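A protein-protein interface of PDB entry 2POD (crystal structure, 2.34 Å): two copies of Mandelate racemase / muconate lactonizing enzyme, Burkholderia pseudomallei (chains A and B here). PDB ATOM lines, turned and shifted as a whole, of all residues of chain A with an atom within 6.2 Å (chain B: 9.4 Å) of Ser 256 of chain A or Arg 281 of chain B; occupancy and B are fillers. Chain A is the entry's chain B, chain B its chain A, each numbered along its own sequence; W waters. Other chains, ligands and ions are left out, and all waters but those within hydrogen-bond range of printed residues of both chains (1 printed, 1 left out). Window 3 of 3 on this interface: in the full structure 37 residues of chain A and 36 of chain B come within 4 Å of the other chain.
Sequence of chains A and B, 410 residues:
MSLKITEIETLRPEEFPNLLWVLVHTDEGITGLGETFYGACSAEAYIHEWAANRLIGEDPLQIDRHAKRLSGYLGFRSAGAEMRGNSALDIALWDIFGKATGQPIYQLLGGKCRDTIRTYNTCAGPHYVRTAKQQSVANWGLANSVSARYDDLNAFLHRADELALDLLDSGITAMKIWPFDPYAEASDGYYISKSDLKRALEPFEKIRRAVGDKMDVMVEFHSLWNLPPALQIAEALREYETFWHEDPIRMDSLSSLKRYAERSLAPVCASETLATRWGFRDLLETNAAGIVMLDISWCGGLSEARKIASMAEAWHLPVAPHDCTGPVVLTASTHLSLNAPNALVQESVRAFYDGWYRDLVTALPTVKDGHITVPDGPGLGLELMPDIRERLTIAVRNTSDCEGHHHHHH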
ATOM      1  N   LEU A 227      17.360 -15.746 -32.496  1.00  0.00           N
ATOM      2  CA  LEU A 227      16.486 -14.834 -31.770  1.00  0.00           C
ATOM      3  C   LEU A 227      16.947 -13.375 -31.603  1.00  0.00           C
ATOM      4  O   LEU A 227      16.226 -12.481 -32.047  1.00  0.00           O
ATOM      5  CB  LEU A 227      15.934 -15.445 -30.481  1.00  0.00           C
ATOM      6  CG  LEU A 227      14.847 -14.633 -29.782  1.00  0.00           C
ATOM      7  CD1 LEU A 227      13.477 -14.813 -30.426  1.00  0.00           C
ATOM      8  CD2 LEU A 227      14.813 -14.995 -28.317  1.00  0.00           C
ATOM      9  N   ILE A 249      12.344 -16.626 -37.659  1.00  0.00           N
ATOM     10  CA  ILE A 249      13.252 -17.629 -37.098  1.00  0.00           C
ATOM     11  C   ILE A 249      12.880 -18.987 -37.679  1.00  0.00           C
ATOM     12  O   ILE A 249      11.817 -19.128 -38.286  1.00  0.00           O
ATOM     13  CB  ILE A 249      13.186 -17.691 -35.532  1.00  0.00           C
ATOM     14  CG1 ILE A 249      11.825 -18.236 -35.046  1.00  0.00           C
ATOM     15  CG2 ILE A 249      13.507 -16.328 -34.917  1.00  0.00           C
ATOM     16  CD1 ILE A 249      11.825 -18.802 -33.624  1.00  0.00           C
ATOM     17  N   ASP A 252      11.278 -24.828 -35.912  1.00  0.00           N
ATOM     18  CA  ASP A 252      11.608 -26.180 -35.464  1.00  0.00           C
ATOM     19  C   ASP A 252      10.896 -26.493 -34.150  1.00  0.00           C
ATOM     20  O   ASP A 252       9.956 -27.287 -34.135  1.00  0.00           O
ATOM     21  CB  ASP A 252      13.126 -26.403 -35.374  1.00  0.00           C
ATOM     22  CG  ASP A 252      13.903 -25.129 -35.036  1.00  0.00           C
ATOM     23  OD1 ASP A 252      13.329 -24.246 -34.362  1.00  0.00           O
ATOM     24  OD2 ASP A 252      15.094 -25.019 -35.427  1.00  0.00           O
ATOM     25  N   SER A 253      11.311 -25.857 -33.058  1.00  0.00           N
ATOM     26  CA  SER A 253      10.446 -25.782 -31.878  1.00  0.00           C
ATOM     27  C   SER A 253       9.745 -24.439 -31.770  1.00  0.00           C
ATOM     28  O   SER A 253      10.375 -23.383 -31.791  1.00  0.00           O
ATOM     29  CB  SER A 253      11.170 -26.166 -30.579  1.00  0.00           C
ATOM     30  OG  SER A 253      12.456 -25.608 -30.509  1.00  0.00           O
ATOM     31  N   LEU A 254       8.423 -24.499 -31.668  1.00  0.00           N
ATOM     32  CA  LEU A 254       7.568 -23.375 -32.011  1.00  0.00           C
ATOM     33  C   LEU A 254       7.343 -22.464 -30.806  1.00  0.00           C
ATOM     34  O   LEU A 254       7.020 -21.286 -30.960  1.00  0.00           O
ATOM     35  CB  LEU A 254       6.238 -23.896 -32.569  1.00  0.00           C
ATOM     36  CG  LEU A 254       5.917 -23.741 -34.063  1.00  0.00           C
ATOM     37  CD1 LEU A 254       7.111 -23.342 -34.903  1.00  0.00           C
ATOM     38  CD2 LEU A 254       5.273 -24.988 -34.619  1.00  0.00           C
ATOM     39  N   SER A 255       7.541 -23.024 -29.612  1.00  0.00           N
ATOM     40  CA  SER A 255       7.601 -22.289 -28.338  1.00  0.00           C
ATOM     41  C   SER A 255       8.394 -20.977 -28.341  1.00  0.00           C
ATOM     42  O   SER A 255       8.107 -20.074 -27.553  1.00  0.00           O
ATOM     43  CB  SER A 255       8.160 -23.204 -27.245  1.00  0.00           C
ATOM     44  OG  SER A 255       7.133 -23.620 -26.369  1.00  0.00           O
ATOM     45  N   SER A 256       9.387 -20.883 -29.222  1.00  0.00           N
ATOM     46  CA  SER A 256      10.247 -19.704 -29.310  1.00  0.00           C
ATOM     47  C   SER A 256       9.617 -18.503 -30.039  1.00  0.00           C
ATOM     48  O   SER A 256      10.204 -17.414 -30.070  1.00  0.00           O
ATOM     49  CB  SER A 256      11.578 -20.076 -29.969  1.00  0.00           C
ATOM     50  OG  SER A 256      12.516 -20.552 -29.019  1.00  0.00           O
ATOM     51  N   LEU A 257       8.436 -18.699 -30.620  1.00  0.00           N
ATOM     52  CA  LEU A 257       7.891 -17.741 -31.578  1.00  0.00           C
ATOM     53  C   LEU A 257       7.226 -16.535 -30.930  1.00  0.00           C
ATOM     54  O   LEU A 257       7.268 -15.435 -31.482  1.00  0.00           O
ATOM     55  CB  LEU A 257       6.937 -18.428 -32.554  1.00  0.00           C
ATOM     56  CG  LEU A 257       6.553 -17.683 -33.832  1.00  0.00           C
ATOM     57  CD1 LEU A 257       7.778 -17.222 -34.617  1.00  0.00           C
ATOM     58  CD2 LEU A 257       5.658 -18.559 -34.673  1.00  0.00           C
ATOM     59  N   LYS A 258       6.631 -16.739 -29.754  1.00  0.00           N
ATOM     60  CA  LYS A 258       5.886 -15.682 -29.069  1.00  0.00           C
ATOM     61  C   LYS A 258       6.784 -14.537 -28.623  1.00  0.00           C
ATOM     62  O   LYS A 258       6.356 -13.386 -28.585  1.00  0.00           O
ATOM     63  CB  LYS A 258       5.092 -16.236 -27.883  1.00  0.00           C
ATOM     64  CG  LYS A 258       3.654 -15.705 -27.812  1.00  0.00           C
ATOM     65  CD  LYS A 258       3.526 -14.395 -27.049  1.00  0.00           C
ATOM     66  CE  LYS A 258       2.544 -13.439 -27.732  1.00  0.00           C
ATOM     67  NZ  LYS A 258       1.118 -13.692 -27.365  1.00  0.00           N
ATOM     68  N   ARG A 259       8.029 -14.872 -28.297  1.00  0.00           N
ATOM     69  CA  ARG A 259       9.068 -13.891 -28.051  1.00  0.00           C
ATOM     70  C   ARG A 259       9.348 -12.985 -29.242  1.00  0.00           C
ATOM     71  O   ARG A 259       9.481 -11.774 -29.068  1.00  0.00           O
ATOM     72  CB  ARG A 259      10.337 -14.573 -27.555  1.00  0.00           C
ATOM     73  CG  ARG A 259      10.184 -15.115 -26.137  1.00  0.00           C
ATOM     74  CD  ARG A 259      11.498 -15.553 -25.546  1.00  0.00           C
ATOM     75  NE  ARG A 259      12.418 -14.432 -25.376  1.00  0.00           N
ATOM     76  CZ  ARG A 259      13.697 -14.551 -25.040  1.00  0.00           C
ATOM     77  NH1 ARG A 259      14.228 -15.749 -24.836  1.00  0.00           N
ATOM     78  NH2 ARG A 259      14.449 -13.467 -24.928  1.00  0.00           N
ATOM     79  N   TYR A 260       9.403 -13.555 -30.448  1.00  0.00           N
ATOM     80  CA  TYR A 260       9.474 -12.732 -31.656  1.00  0.00           C
ATOM     81  C   TYR A 260       8.222 -11.887 -31.875  1.00  0.00           C
ATOM     82  O   TYR A 260       8.328 -10.675 -32.090  1.00  0.00           O
ATOM     83  CB  TYR A 260       9.837 -13.533 -32.918  1.00  0.00           C
ATOM     84  CG  TYR A 260      10.002 -12.638 -34.131  1.00  0.00           C
ATOM     85  CD1 TYR A 260       8.900 -12.287 -34.918  1.00  0.00           C
ATOM     86  CD2 TYR A 260      11.245 -12.101 -34.467  1.00  0.00           C
ATOM     87  CE1 TYR A 260       9.028 -11.445 -36.001  1.00  0.00           C
ATOM     88  CE2 TYR A 260      11.383 -11.251 -35.563  1.00  0.00           C
ATOM     89  CZ  TYR A 260      10.266 -10.928 -36.321  1.00  0.00           C
ATOM     90  OH  TYR A 260      10.360 -10.102 -37.410  1.00  0.00           O
ATOM     91  N   ALA A 261       7.049 -12.529 -31.819  1.00  0.00           N
ATOM     92  CA  ALA A 261       5.770 -11.869 -32.107  1.00  0.00           C
ATOM     93  C   ALA A 261       5.499 -10.639 -31.244  1.00  0.00           C
ATOM     94  O   ALA A 261       5.090  -9.595 -31.763  1.00  0.00           O
ATOM     95  CB  ALA A 261       4.631 -12.848 -32.012  1.00  0.00           C
ATOM     96  N   THR A 286       0.786 -21.327 -30.025  1.00  0.00           N
ATOM     97  CA  THR A 286       1.748 -20.296 -29.591  1.00  0.00           C
ATOM     98  C   THR A 286       1.120 -18.917 -29.331  1.00  0.00           C
ATOM     99  O   THR A 286       1.664 -18.131 -28.551  1.00  0.00           O
ATOM    100  CB  THR A 286       2.928 -20.122 -30.575  1.00  0.00           C
ATOM    101  OG1 THR A 286       2.469 -19.529 -31.803  1.00  0.00           O
ATOM    102  CG2 THR A 286       3.598 -21.458 -30.854  1.00  0.00           C
ATOM    103  N   LEU B 254       2.676 -32.655 -29.519  1.00  0.00           N
ATOM    104  CA  LEU B 254       3.150 -33.213 -28.260  1.00  0.00           C
ATOM    105  C   LEU B 254       2.390 -32.690 -27.052  1.00  0.00           C
ATOM    106  O   LEU B 254       2.432 -33.302 -25.996  1.00  0.00           O
ATOM    107  CB  LEU B 254       4.663 -33.014 -28.107  1.00  0.00           C
ATOM    108  CG  LEU B 254       5.514 -33.834 -29.084  1.00  0.00           C
ATOM    109  CD1 LEU B 254       6.977 -33.490 -28.973  1.00  0.00           C
ATOM    110  CD2 LEU B 254       5.308 -35.321 -28.873  1.00  0.00           C
ATOM    111  N   LEU B 274      10.920 -39.149 -33.223  1.00  0.00           N
ATOM    112  CA  LEU B 274      11.229 -37.734 -32.991  1.00  0.00           C
ATOM    113  C   LEU B 274      12.673 -37.482 -33.419  1.00  0.00           C
ATOM    114  O   LEU B 274      13.544 -38.335 -33.209  1.00  0.00           O
ATOM    115  CB  LEU B 274      11.071 -37.417 -31.503  1.00  0.00           C
ATOM    116  CG  LEU B 274      10.157 -36.331 -30.915  1.00  0.00           C
ATOM    117  CD1 LEU B 274       9.044 -35.852 -31.829  1.00  0.00           C
ATOM    118  CD2 LEU B 274       9.586 -36.837 -29.614  1.00  0.00           C
ATOM    119  N   ALA B 275      12.918 -36.319 -34.018  1.00  0.00           N
ATOM    120  CA  ALA B 275      14.249 -35.965 -34.504  1.00  0.00           C
ATOM    121  C   ALA B 275      14.806 -34.685 -33.875  1.00  0.00           C
ATOM    122  O   ALA B 275      14.076 -33.716 -33.670  1.00  0.00           O
ATOM    123  CB  ALA B 275      14.259 -35.872 -36.041  1.00  0.00           C
ATOM    124  N   THR B 276      16.111 -34.704 -33.601  1.00  0.00           N
ATOM    125  CA  THR B 276      16.919 -33.533 -33.177  1.00  0.00           C
ATOM    126  C   THR B 276      16.613 -32.967 -31.792  1.00  0.00           C
ATOM    127  O   THR B 276      15.653 -33.371 -31.135  1.00  0.00           O
ATOM    128  CB  THR B 276      16.995 -32.368 -34.219  1.00  0.00           C
ATOM    129  OG1 THR B 276      15.828 -31.538 -34.110  1.00  0.00           O
ATOM    130  CG2 THR B 276      17.156 -32.891 -35.649  1.00  0.00           C
ATOM    131  N   ARG B 277      17.445 -32.018 -31.370  1.00  0.00           N
ATOM    132  CA  ARG B 277      17.280 -31.328 -30.099  1.00  0.00           C
ATOM    133  C   ARG B 277      15.964 -30.581 -30.021  1.00  0.00           C
ATOM    134  O   ARG B 277      15.369 -30.500 -28.956  1.00  0.00           O
ATOM    135  CB  ARG B 277      18.430 -30.357 -29.874  1.00  0.00           C
ATOM    136  CG  ARG B 277      19.725 -31.016 -29.467  1.00  0.00           C
ATOM    137  CD  ARG B 277      20.868 -30.037 -29.622  1.00  0.00           C
ATOM    138  NE  ARG B 277      21.285 -29.907 -31.015  1.00  0.00           N
ATOM    139  CZ  ARG B 277      22.061 -28.932 -31.481  1.00  0.00           C
ATOM    140  NH1 ARG B 277      22.518 -27.986 -30.668  1.00  0.00           N
ATOM    141  NH2 ARG B 277      22.387 -28.905 -32.767  1.00  0.00           N
ATOM    142  N   TRP B 278      15.520 -30.054 -31.160  1.00  0.00           N
ATOM    143  CA  TRP B 278      14.280 -29.287 -31.268  1.00  0.00           C
ATOM    144  C   TRP B 278      13.025 -30.139 -31.117  1.00  0.00           C
ATOM    145  O   TRP B 278      12.069 -29.729 -30.444  1.00  0.00           O
ATOM    146  CB  TRP B 278      14.261 -28.511 -32.582  1.00  0.00           C
ATOM    147  CG  TRP B 278      15.310 -27.428 -32.609  1.00  0.00           C
ATOM    148  CD1 TRP B 278      15.164 -26.138 -32.192  1.00  0.00           C
ATOM    149  CD2 TRP B 278      16.673 -27.557 -33.039  1.00  0.00           C
ATOM    150  NE1 TRP B 278      16.341 -25.448 -32.357  1.00  0.00           N
ATOM    151  CE2 TRP B 278      17.285 -26.298 -32.868  1.00  0.00           C
ATOM    152  CE3 TRP B 278      17.433 -28.614 -33.553  1.00  0.00           C
ATOM    153  CZ2 TRP B 278      18.628 -26.065 -33.185  1.00  0.00           C
ATOM    154  CZ3 TRP B 278      18.770 -28.380 -33.878  1.00  0.00           C
ATOM    155  CH2 TRP B 278      19.351 -27.114 -33.694  1.00  0.00           C
ATOM    156  N   GLY B 279      13.028 -31.321 -31.734  1.00  0.00           N
ATOM    157  CA  GLY B 279      12.039 -32.354 -31.423  1.00  0.00           C
ATOM    158  C   GLY B 279      12.028 -32.725 -29.950  1.00  0.00           C
ATOM    159  O   GLY B 279      10.968 -32.829 -29.347  1.00  0.00           O
ATOM    160  N   PHE B 280      13.214 -32.886 -29.362  1.00  0.00           N
ATOM    161  CA  PHE B 280      13.312 -33.267 -27.963  1.00  0.00           C
ATOM    162  C   PHE B 280      13.143 -32.162 -26.923  1.00  0.00           C
ATOM    163  O   PHE B 280      12.691 -32.442 -25.815  1.00  0.00           O
ATOM    164  CB  PHE B 280      14.536 -34.147 -27.700  1.00  0.00           C
ATOM    165  CG  PHE B 280      14.373 -35.542 -28.214  1.00  0.00           C
ATOM    166  CD1 PHE B 280      13.799 -36.522 -27.420  1.00  0.00           C
ATOM    167  CD2 PHE B 280      14.758 -35.871 -29.511  1.00  0.00           C
ATOM    168  CE1 PHE B 280      13.631 -37.806 -27.902  1.00  0.00           C
ATOM    169  CE2 PHE B 280      14.605 -37.156 -30.000  1.00  0.00           C
ATOM    170  CZ  PHE B 280      14.039 -38.126 -29.199  1.00  0.00           C
ATOM    171  N   ARG B 281      13.479 -30.921 -27.284  1.00  0.00           N
ATOM    172  CA  ARG B 281      13.044 -29.744 -26.528  1.00  0.00           C
ATOM    173  C   ARG B 281      11.525 -29.707 -26.366  1.00  0.00           C
ATOM    174  O   ARG B 281      11.024 -29.455 -25.274  1.00  0.00           O
ATOM    175  CB  ARG B 281      13.577 -28.435 -27.149  1.00  0.00           C
ATOM    176  CG  ARG B 281      12.557 -27.306 -27.257  1.00  0.00           C
ATOM    177  CD  ARG B 281      12.987 -26.034 -26.583  1.00  0.00           C
ATOM    178  NE  ARG B 281      13.352 -25.006 -27.548  1.00  0.00           N
ATOM    179  CZ  ARG B 281      12.701 -23.857 -27.718  1.00  0.00           C
ATOM    180  NH1 ARG B 281      11.642 -23.570 -26.981  1.00  0.00           N
ATOM    181  NH2 ARG B 281      13.117 -22.987 -28.629  1.00  0.00           N
ATOM    182  N   ASP B 282      10.814 -29.991 -27.454  1.00  0.00           N
ATOM    183  CA  ASP B 282       9.362 -29.980 -27.482  1.00  0.00           C
ATOM    184  C   ASP B 282       8.762 -31.060 -26.588  1.00  0.00           C
ATOM    185  O   ASP B 282       7.728 -30.828 -25.955  1.00  0.00           O
ATOM    186  CB  ASP B 282       8.855 -30.133 -28.914  1.00  0.00           C
ATOM    187  CG  ASP B 282       8.880 -28.825 -29.685  1.00  0.00           C
ATOM    188  OD1 ASP B 282       8.809 -27.756 -29.037  1.00  0.00           O
ATOM    189  OD2 ASP B 282       8.963 -28.860 -30.937  1.00  0.00           O
ATOM    190  N   LEU B 283       9.420 -32.222 -26.543  1.00  0.00           N
ATOM    191  CA  LEU B 283       9.038 -33.319 -25.652  1.00  0.00           C
ATOM    192  C   LEU B 283       9.243 -32.959 -24.183  1.00  0.00           C
ATOM    193  O   LEU B 283       8.377 -33.222 -23.345  1.00  0.00           O
ATOM    194  CB  LEU B 283       9.822 -34.596 -26.005  1.00  0.00           C
ATOM    195  CG  LEU B 283       9.687 -35.858 -25.150  1.00  0.00           C
ATOM    196  CD1 LEU B 283       8.228 -36.305 -25.037  1.00  0.00           C
ATOM    197  CD2 LEU B 283      10.533 -36.970 -25.755  1.00  0.00           C
ATOM    198  N   LEU B 284      10.385 -32.346 -23.881  1.00  0.00           N
ATOM    199  CA  LEU B 284      10.765 -32.070 -22.499  1.00  0.00           C
ATOM    200  C   LEU B 284       9.946 -30.932 -21.894  1.00  0.00           C
ATOM    201  O   LEU B 284       9.804 -30.838 -20.675  1.00  0.00           O
ATOM    202  CB  LEU B 284      12.265 -31.771 -22.400  1.00  0.00           C
ATOM    203  CG  LEU B 284      13.234 -32.938 -22.589  1.00  0.00           C
ATOM    204  CD1 LEU B 284      14.665 -32.441 -22.701  1.00  0.00           C
ATOM    205  CD2 LEU B 284      13.128 -33.922 -21.453  1.00  0.00           C
ATOM    206  N   GLU B 285       9.394 -30.080 -22.749  1.00  0.00           N
ATOM    207  CA  GLU B 285       8.510 -29.020 -22.285  1.00  0.00           C
ATOM    208  C   GLU B 285       7.100 -29.483 -21.883  1.00  0.00           C
ATOM    209  O   GLU B 285       6.422 -28.795 -21.115  1.00  0.00           O
ATOM    210  CB  GLU B 285       8.467 -27.869 -23.291  1.00  0.00           C
ATOM    211  CG  GLU B 285       9.781 -27.080 -23.349  1.00  0.00           C
ATOM    212  CD  GLU B 285       9.760 -25.930 -24.344  1.00  0.00           C
ATOM    213  OE1 GLU B 285       8.851 -25.876 -25.207  1.00  0.00           O
ATOM    214  OE2 GLU B 285      10.669 -25.074 -24.256  1.00  0.00           O
ATOM    215  N   THR B 286       6.666 -30.640 -22.387  1.00  0.00           N
ATOM    216  CA  THR B 286       5.394 -31.257 -21.955  1.00  0.00           C
ATOM    217  C   THR B 286       5.356 -31.670 -20.471  1.00  0.00           C
ATOM    218  O   THR B 286       4.283 -31.703 -19.873  1.00  0.00           O
ATOM    219  CB  THR B 286       4.993 -32.479 -22.817  1.00  0.00           C
ATOM    220  OG1 THR B 286       5.851 -33.592 -22.525  1.00  0.00           O
ATOM    221  CG2 THR B 286       5.074 -32.147 -24.301  1.00  0.00           C
ATOM    222  N   ASN B 287       6.530 -31.954 -19.898  1.00  0.00           N
ATOM    223  CA  ASN B 287       6.679 -32.642 -18.604  1.00  0.00           C
ATOM    224  C   ASN B 287       5.963 -33.992 -18.504  1.00  0.00           C
ATOM    225  O   ASN B 287       5.427 -34.344 -17.456  1.00  0.00           O
ATOM    226  CB  ASN B 287       6.345 -31.731 -17.416  1.00  0.00           C
ATOM    227  CG  ASN B 287       7.324 -30.578 -17.275  1.00  0.00           C
ATOM    228  OD1 ASN B 287       8.458 -30.761 -16.822  1.00  0.00           O
ATOM    229  ND2 ASN B 287       6.889 -29.378 -17.662  1.00  0.00           N
ATOM    230  N   ALA B 288       5.983 -34.747 -19.598  1.00  0.00           N
ATOM    231  CA  ALA B 288       5.182 -35.950 -19.710  1.00  0.00           C
ATOM    232  C   ALA B 288       6.000 -37.223 -19.887  1.00  0.00           C
ATOM    233  O   ALA B 288       5.546 -38.297 -19.509  1.00  0.00           O
ATOM    234  CB  ALA B 288       4.158 -35.802 -20.835  1.00  0.00           C
ATOM    235  N   VAL B 292      13.512 -40.820 -22.227  1.00  0.00           N
ATOM    236  CA  VAL B 292      13.800 -40.244 -23.532  1.00  0.00           C
ATOM    237  C   VAL B 292      14.363 -41.335 -24.447  1.00  0.00           C
ATOM    238  O   VAL B 292      15.463 -41.843 -24.235  1.00  0.00           O
ATOM    239  CB  VAL B 292      14.743 -39.020 -23.392  1.00  0.00           C
ATOM    240  CG1 VAL B 292      15.290 -38.569 -24.737  1.00  0.00           C
ATOM    241  CG2 VAL B 292      14.004 -37.869 -22.698  1.00  0.00           C
ATOM    242  N   GLU B 304      23.308 -35.254 -32.940  1.00  0.00           N
ATOM    243  CA  GLU B 304      22.108 -34.847 -32.209  1.00  0.00           C
ATOM    244  C   GLU B 304      21.871 -35.711 -30.973  1.00  0.00           C
ATOM    245  O   GLU B 304      21.575 -35.188 -29.908  1.00  0.00           O
ATOM    246  CB  GLU B 304      20.870 -34.819 -33.120  1.00  0.00           C
ATOM    247  CG  GLU B 304      20.884 -33.712 -34.165  1.00  0.00           C
ATOM    248  CD  GLU B 304      20.825 -32.304 -33.572  1.00  0.00           C
ATOM    249  OE1 GLU B 304      21.468 -31.390 -34.132  1.00  0.00           O
ATOM    250  OE2 GLU B 304      20.130 -32.101 -32.559  1.00  0.00           O
ATOM    251  N   LYS B 307      23.608 -34.845 -27.773  1.00  0.00           N
ATOM    252  CA  LYS B 307      23.196 -33.598 -27.177  1.00  0.00           C
ATOM    253  C   LYS B 307      21.815 -33.779 -26.571  1.00  0.00           C
ATOM    254  O   LYS B 307      21.544 -33.255 -25.499  1.00  0.00           O
ATOM    255  CB  LYS B 307      23.184 -32.509 -28.245  1.00  0.00           C
ATOM    256  CG  LYS B 307      24.541 -32.245 -28.843  1.00  0.00           C
ATOM    257  CD  LYS B 307      24.466 -31.415 -30.118  1.00  0.00           C
ATOM    258  CE  LYS B 307      25.837 -31.370 -30.791  1.00  0.00           C
ATOM    259  NZ  LYS B 307      25.851 -30.451 -31.964  1.00  0.00           N
ATOM    260  N   ILE B 308      20.967 -34.558 -27.251  1.00  0.00           N
ATOM    261  CA  ILE B 308      19.698 -35.028 -26.694  1.00  0.00           C
ATOM    262  C   ILE B 308      19.871 -35.745 -25.348  1.00  0.00           C
ATOM    263  O   ILE B 308      19.162 -35.439 -24.386  1.00  0.00           O
ATOM    264  CB  ILE B 308      18.904 -35.904 -27.697  1.00  0.00           C
ATOM    265  CG1 ILE B 308      18.466 -35.081 -28.908  1.00  0.00           C
ATOM    266  CG2 ILE B 308      17.647 -36.475 -27.031  1.00  0.00           C
ATOM    267  CD1 ILE B 308      18.252 -35.916 -30.204  1.00  0.00           C
ATOM    268  N   MET B 311      20.844 -33.199 -22.662  1.00  0.00           N
ATOM    269  CA  MET B 311      19.600 -32.486 -22.349  1.00  0.00           C
ATOM    270  C   MET B 311      18.683 -33.276 -21.418  1.00  0.00           C
ATOM    271  O   MET B 311      18.304 -32.780 -20.359  1.00  0.00           O
ATOM    272  CB  MET B 311      18.824 -32.172 -23.623  1.00  0.00           C
ATOM    273  CG  MET B 311      19.271 -30.947 -24.370  1.00  0.00           C
ATOM    274  SD  MET B 311      17.879 -30.378 -25.608  1.00  0.00           S
ATOM    275  CE  MET B 311      16.582 -29.731 -24.335  1.00  0.00           C
ATOM    276  N   ALA B 312      18.312 -34.489 -21.826  1.00  0.00           N
ATOM    277  CA  ALA B 312      17.488 -35.382 -21.000  1.00  0.00           C
ATOM    278  C   ALA B 312      17.958 -35.505 -19.546  1.00  0.00           C
ATOM    279  O   ALA B 312      17.137 -35.525 -18.638  1.00  0.00           O
ATOM    280  CB  ALA B 312      17.383 -36.752 -21.633  1.00  0.00           C
ATOM    281  N   TRP B 315      16.816 -32.914 -17.130  1.00  0.00           N
ATOM    282  CA  TRP B 315      15.414 -33.061 -16.720  1.00  0.00           C
ATOM    283  C   TRP B 315      15.234 -34.313 -15.873  1.00  0.00           C
ATOM    284  O   TRP B 315      14.108 -34.747 -15.630  1.00  0.00           O
ATOM    285  CB  TRP B 315      14.509 -33.136 -17.943  1.00  0.00           C
ATOM    286  CG  TRP B 315      13.982 -31.804 -18.400  1.00  0.00           C
ATOM    287  CD1 TRP B 315      12.713 -31.318 -18.225  1.00  0.00           C
ATOM    288  CD2 TRP B 315      14.704 -30.791 -19.104  1.00  0.00           C
ATOM    289  NE1 TRP B 315      12.606 -30.068 -18.778  1.00  0.00           N
ATOM    290  CE2 TRP B 315      13.808 -29.721 -19.332  1.00  0.00           C
ATOM    291  CE3 TRP B 315      16.022 -30.683 -19.572  1.00  0.00           C
ATOM    292  CZ2 TRP B 315      14.186 -28.555 -20.006  1.00  0.00           C
ATOM    293  CZ3 TRP B 315      16.396 -29.530 -20.252  1.00  0.00           C
ATOM    294  CH2 TRP B 315      15.481 -28.474 -20.450  1.00  0.00           C
HETATM  295  O   HOH W   1       7.358 -27.144 -32.116  1.00  0.00           O
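NE1 of Trp 278 of chain B sits at hydrogen-bond distance from OD2 of Asp 252 of chain A, 3.3 Å away.
The guanidinium group (NH2) of Arg 281 of chain B sits at hydrogen-bond distance from the side-chain hydroxyl (OG) of Ser 256 of chain A (2.5 Å).
The side-chain carboxylate (OE1) of Glu 285 of chain B lies within hydrogen-bond range of the side-chain hydroxyl (OG) of Ser 255 of chain A, 3.1 Å away.
The side-chain hydroxyl (OG) of Ser 253 of chain A is in hydrogen-bond range of the guanidinium group (NE) of Arg 281 of chain B, 3.2 Å away.
The guanidinium group (NH1) of Arg 281 of chain B lies within salt-bridge range of the side-chain carboxylate (OE2) of Glu 285 of chain B.
OG1 of Thr 276 of chain B lies close to N of Trp 278 of chain B, 3.3 Å away.
Asp 282 of chain B touches Asp 252 of chain A (OD2 to O, 3.7 Å).
Ser 253 of chain A touches Trp 278 of chain B (OG to CD1, 3.2 Å).
OD1 of Asp 282 of chain B touches CB of Ser 253 of chain A (3.2 Å).
Ser 255 of chain A touches Arg 281 of chain B.
Printed residues of chain A within 4 Å of Arg 281 of chain B: Ser 253, Ser 255 and Ser 256.
Ser 255 of chain A touches just these residues of chain B: Arg 281 and Glu 285.
Of the printed residues of chain A, Glu 285 of chain B touches Ser 255.
Of the printed residues of chain B, Ser 253 of chain A touches Trp 278, Arg 281 and Asp 282.
Ala 312 of chain B touches none of the printed residues of chain A.
Tyr 260 of chain A touches none of the printed residues of chain B.
The nearest residue of chain B that does not touch Ser 256 of chain A is Glu 285 of chain B (6.4 Å).
Among the printed residues, 8 pairs touch across the chains.
Among the printed residues, no Asp or Glu carboxylate lies within 4 Å of a Lys or Arg side-chain nitrogen of the other chain.
Positions printed for both chains: 254 and 286.
Of the 8 pairs that touch across the chains among the printed residues, none has its exchanged pair printed and touching as well.
Water W1 lies within hydrogen-bond range of OD2 of Asp 282 of chain B, N of Leu 254 of chain A and O of Asp 252 of chain A.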
